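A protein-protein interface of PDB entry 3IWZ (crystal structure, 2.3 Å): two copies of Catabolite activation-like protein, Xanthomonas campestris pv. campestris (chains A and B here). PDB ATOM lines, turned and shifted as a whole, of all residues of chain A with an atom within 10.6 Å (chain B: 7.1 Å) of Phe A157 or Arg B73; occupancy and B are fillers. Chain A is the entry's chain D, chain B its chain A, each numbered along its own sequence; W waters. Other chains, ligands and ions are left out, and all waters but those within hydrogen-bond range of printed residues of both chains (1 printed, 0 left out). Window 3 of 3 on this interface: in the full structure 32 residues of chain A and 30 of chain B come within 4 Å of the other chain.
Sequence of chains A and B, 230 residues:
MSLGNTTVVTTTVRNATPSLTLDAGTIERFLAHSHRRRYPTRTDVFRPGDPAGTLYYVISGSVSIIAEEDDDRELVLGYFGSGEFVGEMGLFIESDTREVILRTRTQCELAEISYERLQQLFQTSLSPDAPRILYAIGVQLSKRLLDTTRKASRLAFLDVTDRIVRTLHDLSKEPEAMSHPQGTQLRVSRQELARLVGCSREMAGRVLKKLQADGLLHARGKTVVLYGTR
Of chain B, only Glu B69, Arg B73, Glu B74 and Leu B75 come within 4 Å of Phe A157. Of chain A, only Phe A157 comes within 4 Å of Arg B73. Glu B69 touches just these residues of chain A: Ser A153 (3.2 Å) and Phe A157 (3.4 Å). Of the printed residues of chain A, Glu B74 touches Phe A157 (3.6 Å). Of chain A, only Ala A152, Ser A153 and Phe A157 come within 4 Å of Leu B75. No residue of chain A comes within 4 Å of Gly B198. Printed residues of chain B within 4 Å of Leu A155: Leu B155. Of the printed residues of chain B, Ala A152 touches Leu B75 and Leu B155. Of the printed residues of chain B, Ser A153 touches Glu B69 and Leu B75. Of the printed residues of chain A, Leu B155 touches Ala A152 and Leu A155. The nearest residue of chain A that does not touch Arg B73 is Ser A153 (6.2 Å). The nearest printed residue of chain B that does not touch Leu A155 is Leu B75 (6.8 Å).
The backbone NH (N) of Arg B73 sits close to the side-chain carboxylate (OD1) of Asp B71 (3.3 Å). The backbone NH (N) of Leu B75 sits at hydrogen-bond distance from the backbone carbonyl oxygen (O) of Ala B67 (2.9 Å). The side-chain carboxylate (OE1) of Glu B74 is in salt-bridge range of the guanidinium group (NE) of Arg B195.
Among the printed residues, merely in contact across the chains: Ala A152 with Leu B155 (3.3 Å), Phe A157 with Glu B69 (3.4 Å), Phe A157 with Glu B74 (3.6 Å), Ala A152 with Leu B75 (3.6 Å), Ser A153 with Leu B75 (3.6 Å), Phe A157 with Arg B73 (3.7 Å), Leu A155 with Leu B155 (3.8 Å) and Phe A157 with Leu B75 (3.9 Å).
The side-chain carboxylate of Glu B69 lies within hydrogen-bond range of the side-chain hydroxyl of Ser A153, at 3.2 Å.
Printed residues of chain A that touch a printed residue of chain B: Ala A152, Ser A153, Leu A155 and Phe A157. Hydrophobic or aromatic side chains of chain A that line the printed part of chain B: Ala A152, Leu A155 and Phe A157. Along chain A the printed residues that touch a printed residue of chain B span positions 152 to 157. Hydrophobic or aromatic side chains of chain B within 4 Å of the printed part of chain A: Leu B75 and Leu B155. Among the printed residues, no Asp or Glu carboxylate lies within 4 Å of a Lys or Arg side-chain nitrogen of the other chain.
Leu A155 touches its own counterpart, Leu B155. Positions printed for both chains: 155 and 197. Of the 9 pairs that touch across the chains among the printed residues, 1 has its exchanged pair printed and touching as well.
Water W1 lies within hydrogen-bond range of the backbone carbonyl oxygen (O) of Phe A157 (3.2 Å) and the guanidinium group (NH1) of Arg B73 (3.3 Å).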
ATOM      1  N   THR A 149     -29.009  14.113 -23.196  1.00  0.00           N
ATOM      2  CA  THR A 149     -27.577  13.980 -23.447  1.00  0.00           C
ATOM      3  C   THR A 149     -27.076  15.304 -24.016  1.00  0.00           C
ATOM      4  O   THR A 149     -25.997  15.794 -23.648  1.00  0.00           O
ATOM      5  CB  THR A 149     -27.280  12.865 -24.460  1.00  0.00           C
ATOM      6  OG1 THR A 149     -27.679  11.608 -23.908  1.00  0.00           O
ATOM      7  CG2 THR A 149     -25.795  12.834 -24.809  1.00  0.00           C
ATOM      8  N   ARG A 150     -27.873  15.891 -24.906  1.00  0.00           N
ATOM      9  CA  ARG A 150     -27.490  17.161 -25.515  1.00  0.00           C
ATOM     10  C   ARG A 150     -27.482  18.284 -24.496  1.00  0.00           C
ATOM     11  O   ARG A 150     -26.613  19.158 -24.534  1.00  0.00           O
ATOM     12  CB  ARG A 150     -28.431  17.521 -26.670  1.00  0.00           C
ATOM     13  CG  ARG A 150     -28.188  16.719 -27.930  1.00  0.00           C
ATOM     14  CD  ARG A 150     -29.370  16.770 -28.893  1.00  0.00           C
ATOM     15  NE  ARG A 150     -29.013  16.116 -30.151  1.00  0.00           N
ATOM     16  CZ  ARG A 150     -29.858  15.892 -31.152  1.00  0.00           C
ATOM     17  NH1 ARG A 150     -31.132  16.265 -31.062  1.00  0.00           N
ATOM     18  NH2 ARG A 150     -29.426  15.289 -32.252  1.00  0.00           N
ATOM     19  N   LYS A 151     -28.441  18.254 -23.574  1.00  0.00           N
ATOM     20  CA  LYS A 151     -28.537  19.288 -22.549  1.00  0.00           C
ATOM     21  C   LYS A 151     -27.308  19.258 -21.651  1.00  0.00           C
ATOM     22  O   LYS A 151     -26.708  20.290 -21.363  1.00  0.00           O
ATOM     23  CB  LYS A 151     -29.797  19.082 -21.706  1.00  0.00           C
ATOM     24  CG  LYS A 151     -30.365  20.365 -21.151  1.00  0.00           C
ATOM     25  CD  LYS A 151     -31.588  20.096 -20.312  1.00  0.00           C
ATOM     26  CE  LYS A 151     -32.244  21.382 -19.851  1.00  0.00           C
ATOM     27  NZ  LYS A 151     -33.198  21.930 -20.860  1.00  0.00           N
ATOM     28  N   ALA A 152     -26.943  18.068 -21.198  1.00  0.00           N
ATOM     29  CA  ALA A 152     -25.781  17.923 -20.341  1.00  0.00           C
ATOM     30  C   ALA A 152     -24.557  18.473 -21.071  1.00  0.00           C
ATOM     31  O   ALA A 152     -23.730  19.167 -20.488  1.00  0.00           O
ATOM     32  CB  ALA A 152     -25.568  16.453 -19.991  1.00  0.00           C
ATOM     33  N   SER A 153     -24.447  18.155 -22.354  1.00  0.00           N
ATOM     34  CA  SER A 153     -23.319  18.624 -23.144  1.00  0.00           C
ATOM     35  C   SER A 153     -23.295  20.154 -23.134  1.00  0.00           C
ATOM     36  O   SER A 153     -22.243  20.772 -22.947  1.00  0.00           O
ATOM     37  CB  SER A 153     -23.432  18.092 -24.570  1.00  0.00           C
ATOM     38  OG  SER A 153     -22.278  18.380 -25.328  1.00  0.00           O
ATOM     39  N   ARG A 154     -24.465  20.760 -23.300  1.00  0.00           N
ATOM     40  CA  ARG A 154     -24.571  22.212 -23.304  1.00  0.00           C
ATOM     41  C   ARG A 154     -24.296  22.833 -21.935  1.00  0.00           C
ATOM     42  O   ARG A 154     -23.624  23.865 -21.834  1.00  0.00           O
ATOM     43  CB  ARG A 154     -25.957  22.648 -23.792  1.00  0.00           C
ATOM     44  CG  ARG A 154     -26.230  22.392 -25.263  1.00  0.00           C
ATOM     45  CD  ARG A 154     -27.427  23.221 -25.746  1.00  0.00           C
ATOM     46  NE  ARG A 154     -28.632  22.928 -24.979  1.00  0.00           N
ATOM     47  CZ  ARG A 154     -29.528  22.022 -25.338  1.00  0.00           C
ATOM     48  NH1 ARG A 154     -29.358  21.342 -26.462  1.00  0.00           N
ATOM     49  NH2 ARG A 154     -30.574  21.771 -24.561  1.00  0.00           N
ATOM     50  N   LEU A 155     -24.822  22.217 -20.884  1.00  0.00           N
ATOM     51  CA  LEU A 155     -24.613  22.727 -19.531  1.00  0.00           C
ATOM     52  C   LEU A 155     -23.153  22.606 -19.116  1.00  0.00           C
ATOM     53  O   LEU A 155     -22.713  23.227 -18.147  1.00  0.00           O
ATOM     54  CB  LEU A 155     -25.492  21.970 -18.529  1.00  0.00           C
ATOM     55  CG  LEU A 155     -26.991  22.188 -18.714  1.00  0.00           C
ATOM     56  CD1 LEU A 155     -27.775  21.273 -17.784  1.00  0.00           C
ATOM     57  CD2 LEU A 155     -27.314  23.643 -18.445  1.00  0.00           C
ATOM     58  N   ALA A 156     -22.399  21.802 -19.850  1.00  0.00           N
ATOM     59  CA  ALA A 156     -20.993  21.612 -19.540  1.00  0.00           C
ATOM     60  C   ALA A 156     -20.053  22.555 -20.279  1.00  0.00           C
ATOM     61  O   ALA A 156     -19.119  23.067 -19.683  1.00  0.00           O
ATOM     62  CB  ALA A 156     -20.586  20.172 -19.823  1.00  0.00           C
ATOM     63  N   PHE A 157     -20.315  22.799 -21.562  1.00  0.00           N
ATOM     64  CA  PHE A 157     -19.421  23.616 -22.386  1.00  0.00           C
ATOM     65  C   PHE A 157     -19.898  24.960 -22.934  1.00  0.00           C
ATOM     66  O   PHE A 157     -19.079  25.756 -23.400  1.00  0.00           O
ATOM     67  CB  PHE A 157     -18.930  22.762 -23.563  1.00  0.00           C
ATOM     68  CG  PHE A 157     -18.370  21.431 -23.149  1.00  0.00           C
ATOM     69  CD1 PHE A 157     -17.151  21.352 -22.477  1.00  0.00           C
ATOM     70  CD2 PHE A 157     -19.076  20.258 -23.398  1.00  0.00           C
ATOM     71  CE1 PHE A 157     -16.646  20.121 -22.055  1.00  0.00           C
ATOM     72  CE2 PHE A 157     -18.580  19.026 -22.979  1.00  0.00           C
ATOM     73  CZ  PHE A 157     -17.362  18.960 -22.306  1.00  0.00           C
ATOM     74  N   LEU A 158     -21.201  25.218 -22.909  1.00  0.00           N
ATOM     75  CA  LEU A 158     -21.720  26.482 -23.425  1.00  0.00           C
ATOM     76  C   LEU A 158     -22.091  27.456 -22.321  1.00  0.00           C
ATOM     77  O   LEU A 158     -22.502  27.053 -21.239  1.00  0.00           O
ATOM     78  CB  LEU A 158     -22.937  26.236 -24.318  1.00  0.00           C
ATOM     79  CG  LEU A 158     -22.695  25.420 -25.592  1.00  0.00           C
ATOM     80  CD1 LEU A 158     -23.987  25.322 -26.388  1.00  0.00           C
ATOM     81  CD2 LEU A 158     -21.601  26.070 -26.425  1.00  0.00           C
ATOM     82  N   ASP A 159     -21.942  28.750 -22.604  1.00  0.00           N
ATOM     83  CA  ASP A 159     -22.257  29.792 -21.630  1.00  0.00           C
ATOM     84  C   ASP A 159     -23.760  30.054 -21.536  1.00  0.00           C
ATOM     85  O   ASP A 159     -24.517  29.728 -22.447  1.00  0.00           O
ATOM     86  CB  ASP A 159     -21.541  31.097 -21.991  1.00  0.00           C
ATOM     87  CG  ASP A 159     -21.931  31.611 -23.359  1.00  0.00           C
ATOM     88  OD1 ASP A 159     -21.212  31.312 -24.341  1.00  0.00           O
ATOM     89  OD2 ASP A 159     -22.969  32.297 -23.455  1.00  0.00           O
ATOM     90  N   VAL A 160     -24.174  30.662 -20.431  1.00  0.00           N
ATOM     91  CA  VAL A 160     -25.575  30.976 -20.179  1.00  0.00           C
ATOM     92  C   VAL A 160     -26.227  31.659 -21.383  1.00  0.00           C
ATOM     93  O   VAL A 160     -27.095  31.079 -22.046  1.00  0.00           O
ATOM     94  CB  VAL A 160     -25.706  31.896 -18.951  1.00  0.00           C
ATOM     95  CG1 VAL A 160     -27.140  31.899 -18.450  1.00  0.00           C
ATOM     96  CG2 VAL A 160     -24.743  31.437 -17.861  1.00  0.00           C
ATOM     97  N   THR A 161     -25.799  32.888 -21.667  1.00  0.00           N
ATOM     98  CA  THR A 161     -26.345  33.647 -22.788  1.00  0.00           C
ATOM     99  C   THR A 161     -26.427  32.740 -24.009  1.00  0.00           C
ATOM    100  O   THR A 161     -27.438  32.711 -24.714  1.00  0.00           O
ATOM    101  CB  THR A 161     -25.462  34.875 -23.127  1.00  0.00           C
ATOM    102  OG1 THR A 161     -24.207  34.442 -23.660  1.00  0.00           O
ATOM    103  CG2 THR A 161     -25.200  35.705 -21.883  1.00  0.00           C
ATOM    104  N   ASP A 162     -25.359  31.987 -24.244  1.00  0.00           N
ATOM    105  CA  ASP A 162     -25.304  31.072 -25.373  1.00  0.00           C
ATOM    106  C   ASP A 162     -26.467  30.074 -25.324  1.00  0.00           C
ATOM    107  O   ASP A 162     -27.200  29.923 -26.301  1.00  0.00           O
ATOM    108  CB  ASP A 162     -23.969  30.323 -25.362  1.00  0.00           C
ATOM    109  CG  ASP A 162     -23.822  29.363 -26.528  1.00  0.00           C
ATOM    110  OD1 ASP A 162     -24.749  28.555 -26.758  1.00  0.00           O
ATOM    111  OD2 ASP A 162     -22.771  29.409 -27.203  1.00  0.00           O
ATOM    112  N   ARG A 163     -26.634  29.399 -24.185  1.00  0.00           N
ATOM    113  CA  ARG A 163     -27.703  28.409 -24.028  1.00  0.00           C
ATOM    114  C   ARG A 163     -29.084  29.046 -24.197  1.00  0.00           C
ATOM    115  O   ARG A 163     -29.968  28.471 -24.826  1.00  0.00           O
ATOM    116  CB  ARG A 163     -27.629  27.722 -22.648  1.00  0.00           C
ATOM    117  CG  ARG A 163     -26.236  27.241 -22.225  1.00  0.00           C
ATOM    118  CD  ARG A 163     -26.267  26.125 -21.155  1.00  0.00           C
ATOM    119  NE  ARG A 163     -26.743  26.532 -19.829  1.00  0.00           N
ATOM    120  CZ  ARG A 163     -25.993  27.120 -18.901  1.00  0.00           C
ATOM    121  NH1 ARG A 163     -24.712  27.385 -19.135  1.00  0.00           N
ATOM    122  NH2 ARG A 163     -26.517  27.437 -17.727  1.00  0.00           N
ATOM    123  N   ARG A 166     -29.961  29.667 -27.925  1.00  0.00           N
ATOM    124  CA  ARG A 166     -30.291  28.386 -28.540  1.00  0.00           C
ATOM    125  C   ARG A 166     -31.715  27.950 -28.186  1.00  0.00           C
ATOM    126  O   ARG A 166     -32.486  27.545 -29.062  1.00  0.00           O
ATOM    127  CB  ARG A 166     -29.298  27.311 -28.082  1.00  0.00           C
ATOM    128  CG  ARG A 166     -27.964  27.282 -28.825  1.00  0.00           C
ATOM    129  CD  ARG A 166     -27.106  26.148 -28.283  1.00  0.00           C
ATOM    130  NE  ARG A 166     -26.137  25.630 -29.248  1.00  0.00           N
ATOM    131  CZ  ARG A 166     -25.045  26.274 -29.647  1.00  0.00           C
ATOM    132  NH1 ARG A 166     -24.769  27.479 -29.168  1.00  0.00           N
ATOM    133  NH2 ARG A 166     -24.218  25.707 -30.517  1.00  0.00           N
ATOM    134  N   VAL A 197     -32.507  26.593 -19.184  1.00  0.00           N
ATOM    135  CA  VAL A 197     -31.059  26.598 -19.395  1.00  0.00           C
ATOM    136  C   VAL A 197     -30.251  26.300 -18.146  1.00  0.00           C
ATOM    137  O   VAL A 197     -29.034  26.203 -18.210  1.00  0.00           O
ATOM    138  CB  VAL A 197     -30.571  27.953 -19.963  1.00  0.00           C
ATOM    139  CG1 VAL A 197     -31.300  28.265 -21.254  1.00  0.00           C
ATOM    140  CG2 VAL A 197     -30.781  29.058 -18.943  1.00  0.00           C
ATOM    141  N   ILE B  66     -19.660   8.652 -25.148  1.00  0.00           N
ATOM    142  CA  ILE B  66     -19.163  10.009 -24.993  1.00  0.00           C
ATOM    143  C   ILE B  66     -19.794  11.046 -25.906  1.00  0.00           C
ATOM    144  O   ILE B  66     -19.925  10.822 -27.108  1.00  0.00           O
ATOM    145  CB  ILE B  66     -17.654  10.034 -25.261  1.00  0.00           C
ATOM    146  CG1 ILE B  66     -16.977   8.885 -24.496  1.00  0.00           C
ATOM    147  CG2 ILE B  66     -17.076  11.410 -24.904  1.00  0.00           C
ATOM    148  CD1 ILE B  66     -15.463   8.739 -24.748  1.00  0.00           C
ATOM    149  N   ALA B  67     -20.173  12.182 -25.330  1.00  0.00           N
ATOM    150  CA  ALA B  67     -20.752  13.274 -26.106  1.00  0.00           C
ATOM    151  C   ALA B  67     -19.594  14.161 -26.518  1.00  0.00           C
ATOM    152  O   ALA B  67     -18.721  14.502 -25.708  1.00  0.00           O
ATOM    153  CB  ALA B  67     -21.768  14.066 -25.277  1.00  0.00           C
ATOM    154  N   GLU B  68     -19.601  14.533 -27.786  1.00  0.00           N
ATOM    155  CA  GLU B  68     -18.548  15.343 -28.374  1.00  0.00           C
ATOM    156  C   GLU B  68     -19.020  16.764 -28.625  1.00  0.00           C
ATOM    157  O   GLU B  68     -20.202  16.994 -28.885  1.00  0.00           O
ATOM    158  CB  GLU B  68     -18.129  14.698 -29.696  1.00  0.00           C
ATOM    159  CG  GLU B  68     -16.910  15.291 -30.354  1.00  0.00           C
ATOM    160  CD  GLU B  68     -16.616  14.632 -31.690  1.00  0.00           C
ATOM    161  OE1 GLU B  68     -17.414  14.807 -32.637  1.00  0.00           O
ATOM    162  OE2 GLU B  68     -15.590  13.928 -31.788  1.00  0.00           O
ATOM    163  N   GLU B  69     -18.096  17.717 -28.537  1.00  0.00           N
ATOM    164  CA  GLU B  69     -18.412  19.119 -28.797  1.00  0.00           C
ATOM    165  C   GLU B  69     -17.602  19.638 -29.986  1.00  0.00           C
ATOM    166  O   GLU B  69     -16.635  19.006 -30.415  1.00  0.00           O
ATOM    167  CB  GLU B  69     -18.148  19.981 -27.556  1.00  0.00           C
ATOM    168  CG  GLU B  69     -19.403  20.342 -26.765  1.00  0.00           C
ATOM    169  CD  GLU B  69     -20.491  20.967 -27.632  1.00  0.00           C
ATOM    170  OE1 GLU B  69     -20.152  21.727 -28.566  1.00  0.00           O
ATOM    171  OE2 GLU B  69     -21.688  20.705 -27.370  1.00  0.00           O
ATOM    172  N   ASP B  70     -18.005  20.796 -30.502  1.00  0.00           N
ATOM    173  CA  ASP B  70     -17.383  21.433 -31.666  1.00  0.00           C
ATOM    174  C   ASP B  70     -15.891  21.741 -31.548  1.00  0.00           C
ATOM    175  O   ASP B  70     -15.198  21.937 -32.554  1.00  0.00           O
ATOM    176  CB  ASP B  70     -18.140  22.726 -31.992  1.00  0.00           C
ATOM    177  CG  ASP B  70     -19.658  22.545 -31.955  1.00  0.00           C
ATOM    178  OD1 ASP B  70     -20.171  21.636 -32.648  1.00  0.00           O
ATOM    179  OD2 ASP B  70     -20.333  23.313 -31.229  1.00  0.00           O
ATOM    180  N   ASP B  71     -15.400  21.791 -30.316  1.00  0.00           N
ATOM    181  CA  ASP B  71     -13.997  22.083 -30.051  1.00  0.00           C
ATOM    182  C   ASP B  71     -13.260  20.818 -29.613  1.00  0.00           C
ATOM    183  O   ASP B  71     -12.197  20.877 -28.982  1.00  0.00           O
ATOM    184  CB  ASP B  71     -13.916  23.157 -28.966  1.00  0.00           C
ATOM    185  CG  ASP B  71     -14.944  22.942 -27.859  1.00  0.00           C
ATOM    186  OD1 ASP B  71     -14.776  21.991 -27.069  1.00  0.00           O
ATOM    187  OD2 ASP B  71     -15.928  23.714 -27.790  1.00  0.00           O
ATOM    188  N   ASP B  72     -13.839  19.673 -29.966  1.00  0.00           N
ATOM    189  CA  ASP B  72     -13.287  18.372 -29.622  1.00  0.00           C
ATOM    190  C   ASP B  72     -13.221  18.116 -28.111  1.00  0.00           C
ATOM    191  O   ASP B  72     -12.366  17.363 -27.634  1.00  0.00           O
ATOM    192  CB  ASP B  72     -11.900  18.190 -30.252  1.00  0.00           C
ATOM    193  CG  ASP B  72     -11.968  17.739 -31.714  1.00  0.00           C
ATOM    194  OD1 ASP B  72     -12.052  18.604 -32.619  1.00  0.00           O
ATOM    195  OD2 ASP B  72     -11.946  16.508 -31.953  1.00  0.00           O
ATOM    196  N   ARG B  73     -14.122  18.746 -27.358  1.00  0.00           N
ATOM    197  CA  ARG B  73     -14.165  18.538 -25.915  1.00  0.00           C
ATOM    198  C   ARG B  73     -15.177  17.430 -25.626  1.00  0.00           C
ATOM    199  O   ARG B  73     -16.267  17.410 -26.200  1.00  0.00           O
ATOM    200  CB  ARG B  73     -14.547  19.826 -25.194  1.00  0.00           C
ATOM    201  CG  ARG B  73     -13.410  20.356 -24.336  1.00  0.00           C
ATOM    202  CD  ARG B  73     -13.690  21.743 -23.813  1.00  0.00           C
ATOM    203  NE  ARG B  73     -12.638  22.192 -22.903  1.00  0.00           N
ATOM    204  CZ  ARG B  73     -12.585  23.403 -22.357  1.00  0.00           C
ATOM    205  NH1 ARG B  73     -13.532  24.299 -22.630  1.00  0.00           N
ATOM    206  NH2 ARG B  73     -11.589  23.714 -21.532  1.00  0.00           N
ATOM    207  N   GLU B  74     -14.818  16.513 -24.733  1.00  0.00           N
ATOM    208  CA  GLU B  74     -15.686  15.377 -24.441  1.00  0.00           C
ATOM    209  C   GLU B  74     -16.390  15.344 -23.082  1.00  0.00           C
ATOM    210  O   GLU B  74     -15.834  15.756 -22.063  1.00  0.00           O
ATOM    211  CB  GLU B  74     -14.890  14.071 -24.579  1.00  0.00           C
ATOM    212  CG  GLU B  74     -13.998  13.957 -25.804  1.00  0.00           C
ATOM    213  CD  GLU B  74     -13.290  12.606 -25.889  1.00  0.00           C
ATOM    214  OE1 GLU B  74     -12.879  12.065 -24.832  1.00  0.00           O
ATOM    215  OE2 GLU B  74     -13.134  12.087 -27.015  1.00  0.00           O
ATOM    216  N   LEU B  75     -17.613  14.821 -23.091  1.00  0.00           N
ATOM    217  CA  LEU B  75     -18.411  14.643 -21.880  1.00  0.00           C
ATOM    218  C   LEU B  75     -18.762  13.145 -21.781  1.00  0.00           C
ATOM    219  O   LEU B  75     -19.617  12.643 -22.513  1.00  0.00           O
ATOM    220  CB  LEU B  75     -19.706  15.477 -21.936  1.00  0.00           C
ATOM    221  CG  LEU B  75     -20.605  15.269 -20.706  1.00  0.00           C
ATOM    222  CD1 LEU B  75     -19.798  15.591 -19.461  1.00  0.00           C
ATOM    223  CD2 LEU B  75     -21.846  16.148 -20.769  1.00  0.00           C
ATOM    224  N   VAL B  76     -18.093  12.427 -20.893  1.00  0.00           N
ATOM    225  CA  VAL B  76     -18.379  11.008 -20.752  1.00  0.00           C
ATOM    226  C   VAL B  76     -19.724  10.832 -20.067  1.00  0.00           C
ATOM    227  O   VAL B  76     -19.942  11.347 -18.981  1.00  0.00           O
ATOM    228  CB  VAL B  76     -17.272  10.281 -19.952  1.00  0.00           C
ATOM    229  CG1 VAL B  76     -17.581   8.792 -19.859  1.00  0.00           C
ATOM    230  CG2 VAL B  76     -15.932  10.484 -20.633  1.00  0.00           C
ATOM    231  N   LEU B 155     -24.467  19.331 -13.527  1.00  0.00           N
ATOM    232  CA  LEU B 155     -23.712  20.245 -14.363  1.00  0.00           C
ATOM    233  C   LEU B 155     -24.306  21.658 -14.290  1.00  0.00           C
ATOM    234  O   LEU B 155     -23.608  22.650 -14.480  1.00  0.00           O
ATOM    235  CB  LEU B 155     -23.710  19.746 -15.810  1.00  0.00           C
ATOM    236  CG  LEU B 155     -22.759  18.579 -16.087  1.00  0.00           C
ATOM    237  CD1 LEU B 155     -23.086  17.971 -17.436  1.00  0.00           C
ATOM    238  CD2 LEU B 155     -21.304  19.068 -16.041  1.00  0.00           C
ATOM    239  N   ALA B 194     -11.887  14.339 -15.480  1.00  0.00           N
ATOM    240  CA  ALA B 194     -12.160  15.578 -16.176  1.00  0.00           C
ATOM    241  C   ALA B 194     -13.280  15.369 -17.202  1.00  0.00           C
ATOM    242  O   ALA B 194     -14.154  16.216 -17.363  1.00  0.00           O
ATOM    243  CB  ALA B 194     -10.890  16.067 -16.872  1.00  0.00           C
ATOM    244  N   ARG B 195     -13.241  14.235 -17.892  1.00  0.00           N
ATOM    245  CA  ARG B 195     -14.240  13.930 -18.905  1.00  0.00           C
ATOM    246  C   ARG B 195     -15.604  13.651 -18.292  1.00  0.00           C
ATOM    247  O   ARG B 195     -16.627  13.972 -18.880  1.00  0.00           O
ATOM    248  CB  ARG B 195     -13.811  12.725 -19.762  1.00  0.00           C
ATOM    249  CG  ARG B 195     -12.483  12.862 -20.508  1.00  0.00           C
ATOM    250  CD  ARG B 195     -12.346  11.770 -21.592  1.00  0.00           C
ATOM    251  NE  ARG B 195     -11.013  11.687 -22.196  1.00  0.00           N
ATOM    252  CZ  ARG B 195     -10.027  10.894 -21.769  1.00  0.00           C
ATOM    253  NH1 ARG B 195     -10.205  10.095 -20.721  1.00  0.00           N
ATOM    254  NH2 ARG B 195      -8.856  10.885 -22.401  1.00  0.00           N
ATOM    255  N   VAL B 197     -16.928  14.973 -15.494  1.00  0.00           N
ATOM    256  CA  VAL B 197     -17.605  16.125 -14.919  1.00  0.00           C
ATOM    257  C   VAL B 197     -17.496  17.397 -15.728  1.00  0.00           C
ATOM    258  O   VAL B 197     -17.887  18.471 -15.273  1.00  0.00           O
ATOM    259  CB  VAL B 197     -17.083  16.394 -13.516  1.00  0.00           C
ATOM    260  CG1 VAL B 197     -17.318  15.169 -12.660  1.00  0.00           C
ATOM    261  CG2 VAL B 197     -15.591  16.745 -13.578  1.00  0.00           C
ATOM    262  N   GLY B 198     -16.960  17.277 -16.931  1.00  0.00           N
ATOM    263  CA  GLY B 198     -16.834  18.449 -17.767  1.00  0.00           C
ATOM    264  C   GLY B 198     -16.023  19.566 -17.150  1.00  0.00           C
ATOM    265  O   GLY B 198     -16.524  20.678 -16.969  1.00  0.00           O
ATOM    266  N   CYS B 199     -14.782  19.269 -16.782  1.00  0.00           N
ATOM    267  CA  CYS B 199     -13.890  20.294 -16.256  1.00  0.00           C
ATOM    268  C   CYS B 199     -12.558  20.011 -16.931  1.00  0.00           C
ATOM    269  O   CYS B 199     -12.426  19.001 -17.627  1.00  0.00           O
ATOM    270  CB  CYS B 199     -13.774  20.229 -14.726  1.00  0.00           C
ATOM    271  SG  CYS B 199     -12.791  18.891 -14.026  1.00  0.00           S
ATOM    272  N   SER B 200     -11.579  20.893 -16.758  1.00  0.00           N
ATOM    273  CA  SER B 200     -10.275  20.687 -17.384  1.00  0.00           C
ATOM    274  C   SER B 200      -9.519  19.608 -16.621  1.00  0.00           C
ATOM    275  O   SER B 200      -9.862  19.303 -15.481  1.00  0.00           O
ATOM    276  CB  SER B 200      -9.458  21.990 -17.385  1.00  0.00           C
ATOM    277  OG  SER B 200      -9.051  22.336 -16.076  1.00  0.00           O
ATOM    278  N   ARG B 201      -8.495  19.031 -17.248  1.00  0.00           N
ATOM    279  CA  ARG B 201      -7.707  17.993 -16.594  1.00  0.00           C
ATOM    280  C   ARG B 201      -7.032  18.575 -15.362  1.00  0.00           C
ATOM    281  O   ARG B 201      -7.030  17.965 -14.293  1.00  0.00           O
ATOM    282  CB  ARG B 201      -6.620  17.440 -17.524  1.00  0.00           C
ATOM    283  CG  ARG B 201      -5.799  16.354 -16.846  1.00  0.00           C
ATOM    284  CD  ARG B 201      -4.461  16.074 -17.495  1.00  0.00           C
ATOM    285  NE  ARG B 201      -3.554  15.554 -16.473  1.00  0.00           N
ATOM    286  CZ  ARG B 201      -3.007  16.303 -15.515  1.00  0.00           C
ATOM    287  NH1 ARG B 201      -3.255  17.606 -15.458  1.00  0.00           N
ATOM    288  NH2 ARG B 201      -2.247  15.749 -14.582  1.00  0.00           N
HETATM  289  O   HOH W   1     -16.326  24.471 -24.349  1.00  0.00           O
